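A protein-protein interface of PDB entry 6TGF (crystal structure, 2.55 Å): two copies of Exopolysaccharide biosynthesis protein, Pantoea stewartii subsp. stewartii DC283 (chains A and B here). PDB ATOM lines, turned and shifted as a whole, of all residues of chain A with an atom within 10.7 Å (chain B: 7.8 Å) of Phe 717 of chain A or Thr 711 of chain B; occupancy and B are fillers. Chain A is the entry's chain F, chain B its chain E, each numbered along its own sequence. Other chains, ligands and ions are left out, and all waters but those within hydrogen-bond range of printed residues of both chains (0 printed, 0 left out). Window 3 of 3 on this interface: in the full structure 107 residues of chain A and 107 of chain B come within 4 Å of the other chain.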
ATOM      1  N   THR A 711     -34.781   4.171  12.762  1.00  0.00           N
ATOM      2  CA  THR A 711     -35.449   4.637  11.515  1.00  0.00           C
ATOM      3  C   THR A 711     -34.596   5.696  10.798  1.00  0.00           C
ATOM      4  O   THR A 711     -35.004   6.124   9.699  1.00  0.00           O
ATOM      5  CB  THR A 711     -36.847   5.191  11.825  1.00  0.00           C
ATOM      6  OG1 THR A 711     -37.435   4.376  12.839  1.00  0.00           O
ATOM      7  CG2 THR A 711     -37.758   5.231  10.618  1.00  0.00           C
ATOM      8  N   ARG A 712     -33.458   6.091  11.382  1.00  0.00           N
ATOM      9  CA  ARG A 712     -32.618   7.230  10.918  1.00  0.00           C
ATOM     10  C   ARG A 712     -32.185   7.008   9.459  1.00  0.00           C
ATOM     11  O   ARG A 712     -32.377   7.937   8.651  1.00  0.00           O
ATOM     12  CB  ARG A 712     -31.429   7.430  11.864  1.00  0.00           C
ATOM     13  CG  ARG A 712     -31.831   7.905  13.255  1.00  0.00           C
ATOM     14  CD  ARG A 712     -30.676   8.418  14.097  1.00  0.00           C
ATOM     15  NE  ARG A 712     -29.995   7.362  14.840  1.00  0.00           N
ATOM     16  CZ  ARG A 712     -28.959   6.648  14.403  1.00  0.00           C
ATOM     17  NH1 ARG A 712     -28.452   6.854  13.198  1.00  0.00           N
ATOM     18  NH2 ARG A 712     -28.432   5.717  15.179  1.00  0.00           N
ATOM     19  N   LYS A 713     -31.635   5.832   9.131  1.00  0.00           N
ATOM     20  CA  LYS A 713     -31.255   5.458   7.737  1.00  0.00           C
ATOM     21  C   LYS A 713     -30.992   3.956   7.633  1.00  0.00           C
ATOM     22  O   LYS A 713     -30.632   3.321   8.623  1.00  0.00           O
ATOM     23  CB  LYS A 713     -30.014   6.229   7.282  1.00  0.00           C
ATOM     24  CG  LYS A 713     -28.745   5.945   8.073  1.00  0.00           C
ATOM     25  CD  LYS A 713     -27.532   6.631   7.497  1.00  0.00           C
ATOM     26  CE  LYS A 713     -26.314   6.529   8.388  1.00  0.00           C
ATOM     27  NZ  LYS A 713     -25.201   7.365   7.881  1.00  0.00           N
ATOM     28  N   PRO A 714     -31.163   3.346   6.433  1.00  0.00           N
ATOM     29  CA  PRO A 714     -30.938   1.911   6.248  1.00  0.00           C
ATOM     30  C   PRO A 714     -29.572   1.446   6.775  1.00  0.00           C
ATOM     31  O   PRO A 714     -28.593   2.134   6.546  1.00  0.00           O
ATOM     32  CB  PRO A 714     -31.021   1.723   4.726  1.00  0.00           C
ATOM     33  CG  PRO A 714     -31.925   2.845   4.264  1.00  0.00           C
ATOM     34  CD  PRO A 714     -31.614   4.001   5.193  1.00  0.00           C
ATOM     35  N   GLU A 715     -29.548   0.298   7.462  1.00  0.00           N
ATOM     36  CA  GLU A 715     -28.334  -0.294   8.087  1.00  0.00           C
ATOM     37  C   GLU A 715     -27.420  -0.851   6.989  1.00  0.00           C
ATOM     38  O   GLU A 715     -26.198  -0.618   7.066  1.00  0.00           O
ATOM     39  CB  GLU A 715     -28.716  -1.393   9.081  1.00  0.00           C
ATOM     40  CG  GLU A 715     -27.556  -1.862   9.945  1.00  0.00           C
ATOM     41  CD  GLU A 715     -27.686  -3.277  10.485  1.00  0.00           C
ATOM     42  OE1 GLU A 715     -26.664  -3.989  10.521  1.00  0.00           O
ATOM     43  OE2 GLU A 715     -28.807  -3.662  10.870  1.00  0.00           O
ATOM     44  N   GLY A 716     -27.993  -1.569   6.018  1.00  0.00           N
ATOM     45  CA  GLY A 716     -27.261  -2.157   4.880  1.00  0.00           C
ATOM     46  C   GLY A 716     -28.172  -2.436   3.696  1.00  0.00           C
ATOM     47  O   GLY A 716     -29.314  -1.935   3.694  1.00  0.00           O
ATOM     48  N   PHE A 717     -27.672  -3.200   2.717  1.00  0.00           N
ATOM     49  CA  PHE A 717     -28.380  -3.562   1.461  1.00  0.00           C
ATOM     50  C   PHE A 717     -27.975  -4.973   1.018  1.00  0.00           C
ATOM     51  O   PHE A 717     -26.919  -5.467   1.462  1.00  0.00           O
ATOM     52  CB  PHE A 717     -28.064  -2.553   0.353  1.00  0.00           C
ATOM     53  CG  PHE A 717     -28.404  -1.121   0.683  1.00  0.00           C
ATOM     54  CD1 PHE A 717     -29.658  -0.606   0.399  1.00  0.00           C
ATOM     55  CD2 PHE A 717     -27.468  -0.290   1.279  1.00  0.00           C
ATOM     56  CE1 PHE A 717     -29.970   0.711   0.703  1.00  0.00           C
ATOM     57  CE2 PHE A 717     -27.782   1.026   1.585  1.00  0.00           C
ATOM     58  CZ  PHE A 717     -29.032   1.523   1.296  1.00  0.00           C
ATOM     59  N   VAL A 718     -28.800  -5.591   0.165  1.00  0.00           N
ATOM     60  CA  VAL A 718     -28.509  -6.887  -0.522  1.00  0.00           C
ATOM     61  C   VAL A 718     -28.968  -6.779  -1.982  1.00  0.00           C
ATOM     62  O   VAL A 718     -30.026  -6.163  -2.226  1.00  0.00           O
ATOM     63  CB  VAL A 718     -29.167  -8.084   0.195  1.00  0.00           C
ATOM     64  CG1 VAL A 718     -28.531  -8.343   1.552  1.00  0.00           C
ATOM     65  CG2 VAL A 718     -30.675  -7.923   0.333  1.00  0.00           C
ATOM     66  N   SER A 719     -28.189  -7.345  -2.910  1.00  0.00           N
ATOM     67  CA  SER A 719     -28.459  -7.336  -4.374  1.00  0.00           C
ATOM     68  C   SER A 719     -29.684  -8.206  -4.674  1.00  0.00           C
ATOM     69  O   SER A 719     -29.592  -9.433  -4.495  1.00  0.00           O
ATOM     70  CB  SER A 719     -27.258  -7.803  -5.163  1.00  0.00           C
ATOM     71  OG  SER A 719     -26.279  -6.781  -5.259  1.00  0.00           O
ATOM     72  N   VAL A 720     -30.784  -7.582  -5.104  1.00  0.00           N
ATOM     73  CA  VAL A 720     -32.035  -8.269  -5.543  1.00  0.00           C
ATOM     74  C   VAL A 720     -32.362  -7.794  -6.962  1.00  0.00           C
ATOM     75  O   VAL A 720     -32.291  -6.576  -7.205  1.00  0.00           O
ATOM     76  CB  VAL A 720     -33.197  -8.002  -4.567  1.00  0.00           C
ATOM     77  CG1 VAL A 720     -34.502  -8.625  -5.044  1.00  0.00           C
ATOM     78  CG2 VAL A 720     -32.868  -8.480  -3.161  1.00  0.00           C
ATOM     79  N   ILE A 722     -35.139  -7.160  -8.879  1.00  0.00           N
ATOM     80  CA  ILE A 722     -36.604  -6.866  -8.853  1.00  0.00           C
ATOM     81  C   ILE A 722     -37.060  -6.627 -10.296  1.00  0.00           C
ATOM     82  O   ILE A 722     -36.524  -5.705 -10.939  1.00  0.00           O
ATOM     83  CB  ILE A 722     -36.927  -5.684  -7.915  1.00  0.00           C
ATOM     84  CG1 ILE A 722     -36.476  -5.981  -6.479  1.00  0.00           C
ATOM     85  CG2 ILE A 722     -38.406  -5.327  -7.990  1.00  0.00           C
ATOM     86  CD1 ILE A 722     -36.879  -4.943  -5.453  1.00  0.00           C
ATOM     87  N   THR A 726     -31.233  -5.330 -11.556  1.00  0.00           N
ATOM     88  CA  THR A 726     -30.449  -5.521 -10.305  1.00  0.00           C
ATOM     89  C   THR A 726     -30.495  -4.219  -9.498  1.00  0.00           C
ATOM     90  O   THR A 726     -29.889  -3.225  -9.948  1.00  0.00           O
ATOM     91  CB  THR A 726     -29.001  -5.941 -10.597  1.00  0.00           C
ATOM     92  OG1 THR A 726     -29.025  -7.069 -11.469  1.00  0.00           O
ATOM     93  CG2 THR A 726     -28.222  -6.290  -9.347  1.00  0.00           C
ATOM     94  N   VAL A 727     -31.195  -4.232  -8.360  1.00  0.00           N
ATOM     95  CA  VAL A 727     -31.350  -3.070  -7.435  1.00  0.00           C
ATOM     96  C   VAL A 727     -30.787  -3.471  -6.066  1.00  0.00           C
ATOM     97  O   VAL A 727     -30.338  -4.627  -5.930  1.00  0.00           O
ATOM     98  CB  VAL A 727     -32.820  -2.615  -7.347  1.00  0.00           C
ATOM     99  CG1 VAL A 727     -33.385  -2.278  -8.720  1.00  0.00           C
ATOM    100  CG2 VAL A 727     -33.703  -3.640  -6.651  1.00  0.00           C
ATOM    101  N   ALA A 728     -30.807  -2.548  -5.099  1.00  0.00           N
ATOM    102  CA  ALA A 728     -30.332  -2.755  -3.711  1.00  0.00           C
ATOM    103  C   ALA A 728     -31.525  -2.703  -2.750  1.00  0.00           C
ATOM    104  O   ALA A 728     -32.103  -1.611  -2.585  1.00  0.00           O
ATOM    105  CB  ALA A 728     -29.295  -1.715  -3.361  1.00  0.00           C
ATOM    106  N   LEU A 729     -31.880  -3.845  -2.151  1.00  0.00           N
ATOM    107  CA  LEU A 729     -33.002  -3.962  -1.179  1.00  0.00           C
ATOM    108  C   LEU A 729     -32.532  -3.447   0.179  1.00  0.00           C
ATOM    109  O   LEU A 729     -31.590  -3.990   0.753  1.00  0.00           O
ATOM    110  CB  LEU A 729     -33.462  -5.420  -1.092  1.00  0.00           C
ATOM    111  CG  LEU A 729     -34.789  -5.646  -0.365  1.00  0.00           C
ATOM    112  CD1 LEU A 729     -35.957  -5.100  -1.174  1.00  0.00           C
ATOM    113  CD2 LEU A 729     -35.000  -7.122  -0.061  1.00  0.00           C
ATOM    114  N   PRO A 730     -33.172  -2.394   0.737  1.00  0.00           N
ATOM    115  CA  PRO A 730     -32.749  -1.816   2.010  1.00  0.00           C
ATOM    116  C   PRO A 730     -33.300  -2.584   3.219  1.00  0.00           C
ATOM    117  O   PRO A 730     -34.333  -3.216   3.093  1.00  0.00           O
ATOM    118  CB  PRO A 730     -33.361  -0.411   1.944  1.00  0.00           C
ATOM    119  CG  PRO A 730     -34.663  -0.629   1.205  1.00  0.00           C
ATOM    120  CD  PRO A 730     -34.352  -1.707   0.185  1.00  0.00           C
ATOM    121  N   TYR A 731     -32.593  -2.507   4.348  1.00  0.00           N
ATOM    122  CA  TYR A 731     -33.044  -2.998   5.676  1.00  0.00           C
ATOM    123  C   TYR A 731     -32.502  -2.055   6.754  1.00  0.00           C
ATOM    124  O   TYR A 731     -31.418  -1.474   6.551  1.00  0.00           O
ATOM    125  CB  TYR A 731     -32.619  -4.454   5.890  1.00  0.00           C
ATOM    126  CG  TYR A 731     -31.133  -4.710   5.947  1.00  0.00           C
ATOM    127  CD1 TYR A 731     -30.408  -4.468   7.104  1.00  0.00           C
ATOM    128  CD2 TYR A 731     -30.454  -5.235   4.859  1.00  0.00           C
ATOM    129  CE1 TYR A 731     -29.046  -4.714   7.171  1.00  0.00           C
ATOM    130  CE2 TYR A 731     -29.092  -5.489   4.909  1.00  0.00           C
ATOM    131  CZ  TYR A 731     -28.385  -5.230   6.070  1.00  0.00           C
ATOM    132  OH  TYR A 731     -27.045  -5.477   6.126  1.00  0.00           O
ATOM    133  N   PHE A 732     -33.239  -1.908   7.858  1.00  0.00           N
ATOM    134  CA  PHE A 732     -32.907  -1.003   8.990  1.00  0.00           C
ATOM    135  C   PHE A 732     -32.469  -1.833  10.199  1.00  0.00           C
ATOM    136  O   PHE A 732     -32.835  -3.022  10.283  1.00  0.00           O
ATOM    137  CB  PHE A 732     -34.102  -0.110   9.323  1.00  0.00           C
ATOM    138  CG  PHE A 732     -34.337   1.007   8.339  1.00  0.00           C
ATOM    139  CD1 PHE A 732     -35.294   0.896   7.342  1.00  0.00           C
ATOM    140  CD2 PHE A 732     -33.594   2.172   8.408  1.00  0.00           C
ATOM    141  CE1 PHE A 732     -35.515   1.931   6.447  1.00  0.00           C
ATOM    142  CE2 PHE A 732     -33.816   3.204   7.508  1.00  0.00           C
ATOM    143  CZ  PHE A 732     -34.769   3.082   6.528  1.00  0.00           C
ATOM    144  N   ALA A 733     -31.708  -1.214  11.107  1.00  0.00           N
ATOM    145  CA  ALA A 733     -31.212  -1.838  12.355  1.00  0.00           C
ATOM    146  C   ALA A 733     -32.376  -1.991  13.338  1.00  0.00           C
ATOM    147  O   ALA A 733     -33.296  -1.150  13.313  1.00  0.00           O
ATOM    148  CB  ALA A 733     -30.092  -1.023  12.952  1.00  0.00           C
ATOM    149  N   SER B 701     -29.233 -13.644  -0.319  1.00  0.00           N
ATOM    150  CA  SER B 701     -28.784 -12.959  -1.561  1.00  0.00           C
ATOM    151  C   SER B 701     -27.406 -12.330  -1.326  1.00  0.00           C
ATOM    152  O   SER B 701     -26.960 -12.312  -0.161  1.00  0.00           O
ATOM    153  CB  SER B 701     -29.790 -11.928  -2.001  1.00  0.00           C
ATOM    154  OG  SER B 701     -29.516 -11.492  -3.321  1.00  0.00           O
ATOM    155  N   ARG B 702     -26.764 -11.835  -2.387  1.00  0.00           N
ATOM    156  CA  ARG B 702     -25.426 -11.187  -2.320  1.00  0.00           C
ATOM    157  C   ARG B 702     -25.516  -9.927  -1.452  1.00  0.00           C
ATOM    158  O   ARG B 702     -26.383  -9.077  -1.734  1.00  0.00           O
ATOM    159  CB  ARG B 702     -24.912 -10.820  -3.715  1.00  0.00           C
ATOM    160  CG  ARG B 702     -24.475 -12.012  -4.555  1.00  0.00           C
ATOM    161  CD  ARG B 702     -23.763 -11.597  -5.828  1.00  0.00           C
ATOM    162  NE  ARG B 702     -24.576 -10.734  -6.673  1.00  0.00           N
ATOM    163  CZ  ARG B 702     -24.219 -10.285  -7.873  1.00  0.00           C
ATOM    164  NH1 ARG B 702     -23.048 -10.616  -8.393  1.00  0.00           N
ATOM    165  NH2 ARG B 702     -25.036  -9.503  -8.557  1.00  0.00           N
ATOM    166  N   ALA B 703     -24.654  -9.828  -0.435  1.00  0.00           N
ATOM    167  CA  ALA B 703     -24.491  -8.637   0.432  1.00  0.00           C
ATOM    168  C   ALA B 703     -23.897  -7.493  -0.395  1.00  0.00           C
ATOM    169  O   ALA B 703     -22.987  -7.763  -1.205  1.00  0.00           O
ATOM    170  CB  ALA B 703     -23.618  -8.975   1.616  1.00  0.00           C
ATOM    171  N   LEU B 704     -24.398  -6.269  -0.199  1.00  0.00           N
ATOM    172  CA  LEU B 704     -23.922  -5.042  -0.894  1.00  0.00           C
ATOM    173  C   LEU B 704     -23.232  -4.115   0.112  1.00  0.00           C
ATOM    174  O   LEU B 704     -23.701  -4.029   1.264  1.00  0.00           O
ATOM    175  CB  LEU B 704     -25.107  -4.328  -1.553  1.00  0.00           C
ATOM    176  CG  LEU B 704     -25.464  -4.785  -2.967  1.00  0.00           C
ATOM    177  CD1 LEU B 704     -26.719  -4.079  -3.455  1.00  0.00           C
ATOM    178  CD2 LEU B 704     -24.318  -4.541  -3.937  1.00  0.00           C
ATOM    179  N   SER B 705     -22.163  -3.445  -0.328  1.00  0.00           N
ATOM    180  CA  SER B 705     -21.492  -2.338   0.400  1.00  0.00           C
ATOM    181  C   SER B 705     -22.315  -1.058   0.214  1.00  0.00           C
ATOM    182  O   SER B 705     -22.730  -0.790  -0.931  1.00  0.00           O
ATOM    183  CB  SER B 705     -20.072  -2.154  -0.076  1.00  0.00           C
ATOM    184  OG  SER B 705     -20.041  -1.651  -1.403  1.00  0.00           O
ATOM    185  N   ALA B 706     -22.542  -0.310   1.299  1.00  0.00           N
ATOM    186  CA  ALA B 706     -23.257   0.989   1.305  1.00  0.00           C
ATOM    187  C   ALA B 706     -22.571   1.967   0.341  1.00  0.00           C
ATOM    188  O   ALA B 706     -23.270   2.848  -0.199  1.00  0.00           O
ATOM    189  CB  ALA B 706     -23.310   1.544   2.708  1.00  0.00           C
ATOM    190  N   ASP B 707     -21.257   1.807   0.136  1.00  0.00           N
ATOM    191  CA  ASP B 707     -20.413   2.631  -0.773  1.00  0.00           C
ATOM    192  C   ASP B 707     -20.943   2.564  -2.210  1.00  0.00           C
ATOM    193  O   ASP B 707     -20.902   3.605  -2.895  1.00  0.00           O
ATOM    194  CB  ASP B 707     -18.951   2.176  -0.737  1.00  0.00           C
ATOM    195  CG  ASP B 707     -18.241   2.454   0.577  1.00  0.00           C
ATOM    196  OD1 ASP B 707     -18.930   2.790   1.561  1.00  0.00           O
ATOM    197  OD2 ASP B 707     -17.001   2.330   0.606  1.00  0.00           O
ATOM    198  N   ASN B 708     -21.414   1.391  -2.649  1.00  0.00           N
ATOM    199  CA  ASN B 708     -21.808   1.114  -4.059  1.00  0.00           C
ATOM    200  C   ASN B 708     -23.289   1.448  -4.289  1.00  0.00           C
ATOM    201  O   ASN B 708     -23.750   1.256  -5.430  1.00  0.00           O
ATOM    202  CB  ASN B 708     -21.508  -0.338  -4.447  1.00  0.00           C
ATOM    203  CG  ASN B 708     -20.027  -0.617  -4.597  1.00  0.00           C
ATOM    204  OD1 ASN B 708     -19.499  -1.542  -3.986  1.00  0.00           O
ATOM    205  ND2 ASN B 708     -19.346   0.175  -5.410  1.00  0.00           N
ATOM    206  N   VAL B 709     -23.997   1.949  -3.269  1.00  0.00           N
ATOM    207  CA  VAL B 709     -25.464   2.234  -3.319  1.00  0.00           C
ATOM    208  C   VAL B 709     -25.691   3.749  -3.231  1.00  0.00           C
ATOM    209  O   VAL B 709     -25.080   4.387  -2.351  1.00  0.00           O
ATOM    210  CB  VAL B 709     -26.214   1.489  -2.195  1.00  0.00           C
ATOM    211  CG1 VAL B 709     -27.714   1.748  -2.233  1.00  0.00           C
ATOM    212  CG2 VAL B 709     -25.937  -0.006  -2.229  1.00  0.00           C
ATOM    213  N   ASP B 710     -26.539   4.291  -4.113  1.00  0.00           N
ATOM    214  CA  ASP B 710     -27.092   5.670  -4.030  1.00  0.00           C
ATOM    215  C   ASP B 710     -28.051   5.711  -2.833  1.00  0.00           C
ATOM    216  O   ASP B 710     -29.251   5.430  -3.022  1.00  0.00           O
ATOM    217  CB  ASP B 710     -27.764   6.071  -5.348  1.00  0.00           C
ATOM    218  CG  ASP B 710     -28.225   7.518  -5.415  1.00  0.00           C
ATOM    219  OD1 ASP B 710     -28.310   8.163  -4.352  1.00  0.00           O
ATOM    220  OD2 ASP B 710     -28.504   7.990  -6.536  1.00  0.00           O
ATOM    221  N   THR B 711     -27.528   6.054  -1.652  1.00  0.00           N
ATOM    222  CA  THR B 711     -28.142   5.784  -0.322  1.00  0.00           C
ATOM    223  C   THR B 711     -29.217   6.821   0.041  1.00  0.00           C
ATOM    224  O   THR B 711     -30.062   6.494   0.896  1.00  0.00           O
ATOM    225  CB  THR B 711     -27.072   5.736   0.778  1.00  0.00           C
ATOM    226  OG1 THR B 711     -26.038   6.666   0.456  1.00  0.00           O
ATOM    227  CG2 THR B 711     -26.473   4.358   0.952  1.00  0.00           C
ATOM    228  N   ARG B 712     -29.194   8.011  -0.568  1.00  0.00           N
ATOM    229  CA  ARG B 712     -29.950   9.197  -0.074  1.00  0.00           C
ATOM    230  C   ARG B 712     -31.445   9.099  -0.413  1.00  0.00           C
ATOM    231  O   ARG B 712     -32.234   9.742   0.306  1.00  0.00           O
ATOM    232  CB  ARG B 712     -29.344  10.500  -0.606  1.00  0.00           C
ATOM    233  CG  ARG B 712     -29.411  10.682  -2.115  1.00  0.00           C
ATOM    234  CD  ARG B 712     -28.312  11.614  -2.591  1.00  0.00           C
ATOM    235  NE  ARG B 712     -28.382  11.925  -4.014  1.00  0.00           N
ATOM    236  CZ  ARG B 712     -27.686  11.320  -4.977  1.00  0.00           C
ATOM    237  NH1 ARG B 712     -26.840  10.341  -4.698  1.00  0.00           N
ATOM    238  NH2 ARG B 712     -27.841  11.705  -6.233  1.00  0.00           N
ATOM    239  N   LYS B 713     -31.834   8.340  -1.445  1.00  0.00           N
ATOM    240  CA  LYS B 713     -33.247   8.272  -1.911  1.00  0.00           C
ATOM    241  C   LYS B 713     -33.523   6.927  -2.583  1.00  0.00           C
ATOM    242  O   LYS B 713     -32.681   6.425  -3.325  1.00  0.00           O
ATOM    243  CB  LYS B 713     -33.526   9.431  -2.874  1.00  0.00           C
ATOM    244  CG  LYS B 713     -34.972   9.910  -2.915  1.00  0.00           C
ATOM    245  CD  LYS B 713     -35.329  10.687  -4.165  1.00  0.00           C
ATOM    246  CE  LYS B 713     -35.175   9.870  -5.431  1.00  0.00           C
ATOM    247  NZ  LYS B 713     -36.076  10.344  -6.508  1.00  0.00           N
ATOM    248  N   PRO B 714     -34.699   6.296  -2.343  1.00  0.00           N
ATOM    249  CA  PRO B 714     -35.098   5.098  -3.084  1.00  0.00           C
ATOM    250  C   PRO B 714     -35.326   5.391  -4.577  1.00  0.00           C
ATOM    251  O   PRO B 714     -35.977   6.376  -4.881  1.00  0.00           O
ATOM    252  CB  PRO B 714     -36.405   4.649  -2.409  1.00  0.00           C
ATOM    253  CG  PRO B 714     -36.929   5.893  -1.721  1.00  0.00           C
ATOM    254  CD  PRO B 714     -35.694   6.675  -1.324  1.00  0.00           C
ATOM    255  N   TYR B 731     -36.549   0.119  -3.159  1.00  0.00           N
ATOM    256  CA  TYR B 731     -35.194  -0.328  -3.575  1.00  0.00           C
ATOM    257  C   TYR B 731     -34.360   0.896  -3.966  1.00  0.00           C
ATOM    258  O   TYR B 731     -34.888   1.794  -4.651  1.00  0.00           O
ATOM    259  CB  TYR B 731     -35.270  -1.344  -4.718  1.00  0.00           C
ATOM    260  CG  TYR B 731     -36.076  -0.908  -5.916  1.00  0.00           C
ATOM    261  CD1 TYR B 731     -37.433  -1.178  -5.998  1.00  0.00           C
ATOM    262  CD2 TYR B 731     -35.485  -0.239  -6.977  1.00  0.00           C
ATOM    263  CE1 TYR B 731     -38.182  -0.792  -7.098  1.00  0.00           C
ATOM    264  CE2 TYR B 731     -36.220   0.155  -8.083  1.00  0.00           C
ATOM    265  CZ  TYR B 731     -37.574  -0.122  -8.144  1.00  0.00           C
ATOM    266  OH  TYR B 731     -38.308   0.264  -9.227  1.00  0.00           O
ATOM    267  N   PHE B 732     -33.098   0.922  -3.528  1.00  0.00           N
ATOM    268  CA  PHE B 732     -32.111   1.995  -3.819  1.00  0.00           C
ATOM    269  C   PHE B 732     -31.239   1.549  -4.994  1.00  0.00           C
ATOM    270  O   PHE B 732     -31.056   0.330  -5.183  1.00  0.00           O
ATOM    271  CB  PHE B 732     -31.283   2.316  -2.573  1.00  0.00           C
ATOM    272  CG  PHE B 732     -32.072   2.940  -1.448  1.00  0.00           C
ATOM    273  CD1 PHE B 732     -32.985   2.191  -0.721  1.00  0.00           C
ATOM    274  CD2 PHE B 732     -31.910   4.278  -1.120  1.00  0.00           C
ATOM    275  CE1 PHE B 732     -33.713   2.764   0.309  1.00  0.00           C
ATOM    276  CE2 PHE B 732     -32.639   4.849  -0.088  1.00  0.00           C
ATOM    277  CZ  PHE B 732     -33.540   4.092   0.623  1.00  0.00           C
ATOM    278  N   ALA B 733     -30.730   2.513  -5.765  1.00  0.00           N
ATOM    279  CA  ALA B 733     -29.921   2.279  -6.982  1.00  0.00           C
ATOM    280  C   ALA B 733     -28.503   1.849  -6.593  1.00  0.00           C
ATOM    281  O   ALA B 733     -28.068   2.167  -5.469  1.00  0.00           O
ATOM    282  CB  ALA B 733     -29.897   3.520  -7.839  1.00  0.00           C
ATOM    283  N   ILE B 734     -27.823   1.151  -7.508  1.00  0.00           N
ATOM    284  CA  ILE B 734     -26.387   0.753  -7.413  1.00  0.00           C
ATOM    285  C   ILE B 734     -25.616   1.553  -8.468  1.00  0.00           C
ATOM    286  O   ILE B 734     -26.083   1.592  -9.623  1.00  0.00           O
ATOM    287  CB  ILE B 734     -26.211  -0.766  -7.620  1.00  0.00           C
ATOM    288  CG1 ILE B 734     -27.314  -1.576  -6.928  1.00  0.00           C
ATOM    289  CG2 ILE B 734     -24.816  -1.203  -7.192  1.00  0.00           C
ATOM    290  CD1 ILE B 734     -27.085  -3.073  -6.920  1.00  0.00           C
ATOM    291  N   LYS B 735     -24.485   2.160  -8.093  1.00  0.00           N
ATOM    292  CA  LYS B 735     -23.650   2.993  -9.000  1.00  0.00           C
ATOM    293  C   LYS B 735     -22.349   2.253  -9.329  1.00  0.00           C
ATOM    294  O   LYS B 735     -22.147   1.105  -8.931  1.00  0.00           O
ATOM    295  CB  LYS B 735     -23.366   4.353  -8.359  1.00  0.00           C
ATOM    296  CG  LYS B 735     -24.607   5.172  -8.025  1.00  0.00           C
ATOM    297  CD  LYS B 735     -24.346   6.662  -7.926  1.00  0.00           C
ATOM    298  CE  LYS B 735     -25.583   7.507  -8.154  1.00  0.00           C
ATOM    299  NZ  LYS B 735     -26.135   7.337  -9.521  1.00  0.00           N
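The backbone carbonyl oxygen of Phe 717 of chain A lies within hydrogen-bond range of the backbone NH of Leu 704 of chain B (3.1 Å). The backbone NH (N) of Ser 719 of chain A lies within hydrogen-bond range of the backbone carbonyl oxygen (O) of Arg 702 of chain B (2.8 Å). The backbone NH (N) of Phe 732 of chain B lies within hydrogen-bond range of the backbone carbonyl oxygen (O) of Ala 728 of chain A (2.9 Å). The backbone carbonyl oxygen (O) of Ser 719 of chain A lies close to the side-chain hydroxyl (OG) of Ser 701 of chain B, at 2.4 Å.
The backbone carbonyl oxygen of Val 718 of chain A is in hydrogen-bond range of the backbone NH of Leu 729 of chain A. The backbone NH (N) of Val 727 of chain A lies within hydrogen-bond range of the backbone carbonyl oxygen (O) of Val 720 of chain A (2.8 Å).
Among the printed residues, pairs that only touch across the chains: Ser 719 of chain A with Leu 704 of chain B, Val 718 of chain A with Arg 702 of chain B, Val 727 of chain A with Tyr 731 of chain B, Ala 728 of chain A with Tyr 731 of chain B, Ala 728 of chain A with Leu 704 of chain B, Pro 730 of chain A with Phe 732 of chain B, Phe 717 of chain A with Thr 711 of chain B, Phe 717 of chain A with Phe 732 of chain B, Val 727 of chain A with Ile 734 of chain B, Phe 717 of chain A with Val 709 of chain B, Val 718 of chain A with Leu 704 of chain B, Ile 722 of chain A with Tyr 731 of chain B, Val 727 of chain A with Phe 732 of chain B and Ala 728 of chain A with Val 709 of chain B.
Phe 717 of chain A touches just these residues of chain B: Leu 704 (3.1 Å), Val 709 (3.8 Å), Thr 711 (3.6 Å) and Phe 732 (3.6 Å). Printed residues of chain A within 4 Å of Thr 711 of chain B: Phe 717. No residue of chain B comes within 4 Å of Gly 716 of chain A. Leu 704 of chain B touches just these residues of chain A: Phe 717 (3.1 Å), Val 718 (3.8 Å), Ser 719 (3.1 Å) and Ala 728 (3.5 Å). Of the printed residues of chain A, Val 709 of chain B touches Phe 717 (3.8 Å) and Ala 728 (3.9 Å). Of the printed residues of chain A, Ile 734 of chain B touches Val 727 (3.7 Å). Of the printed residues of chain A, Ser 701 of chain B touches Ser 719.
Printed residues of chain A that touch a printed residue of chain B: Phe 717, Val 718, Ser 719, Ile 722, Val 727, Ala 728 and Pro 730. Along chain A the printed residues that touch a printed residue of chain B span positions 717 to 730. Hydrophobic or aromatic side chains of chain B that line the printed part of chain A: Leu 704, Val 709, Tyr 731, Phe 732 and Ile 734. Among the printed residues, no Asp or Glu carboxylate lies within 4 Å of a Lys or Arg side-chain nitrogen of the other chain.
7 positions are printed for both chains. Of the 18 pairs that touch across the chains among the printed residues, none has its exchanged pair printed and touching as well.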
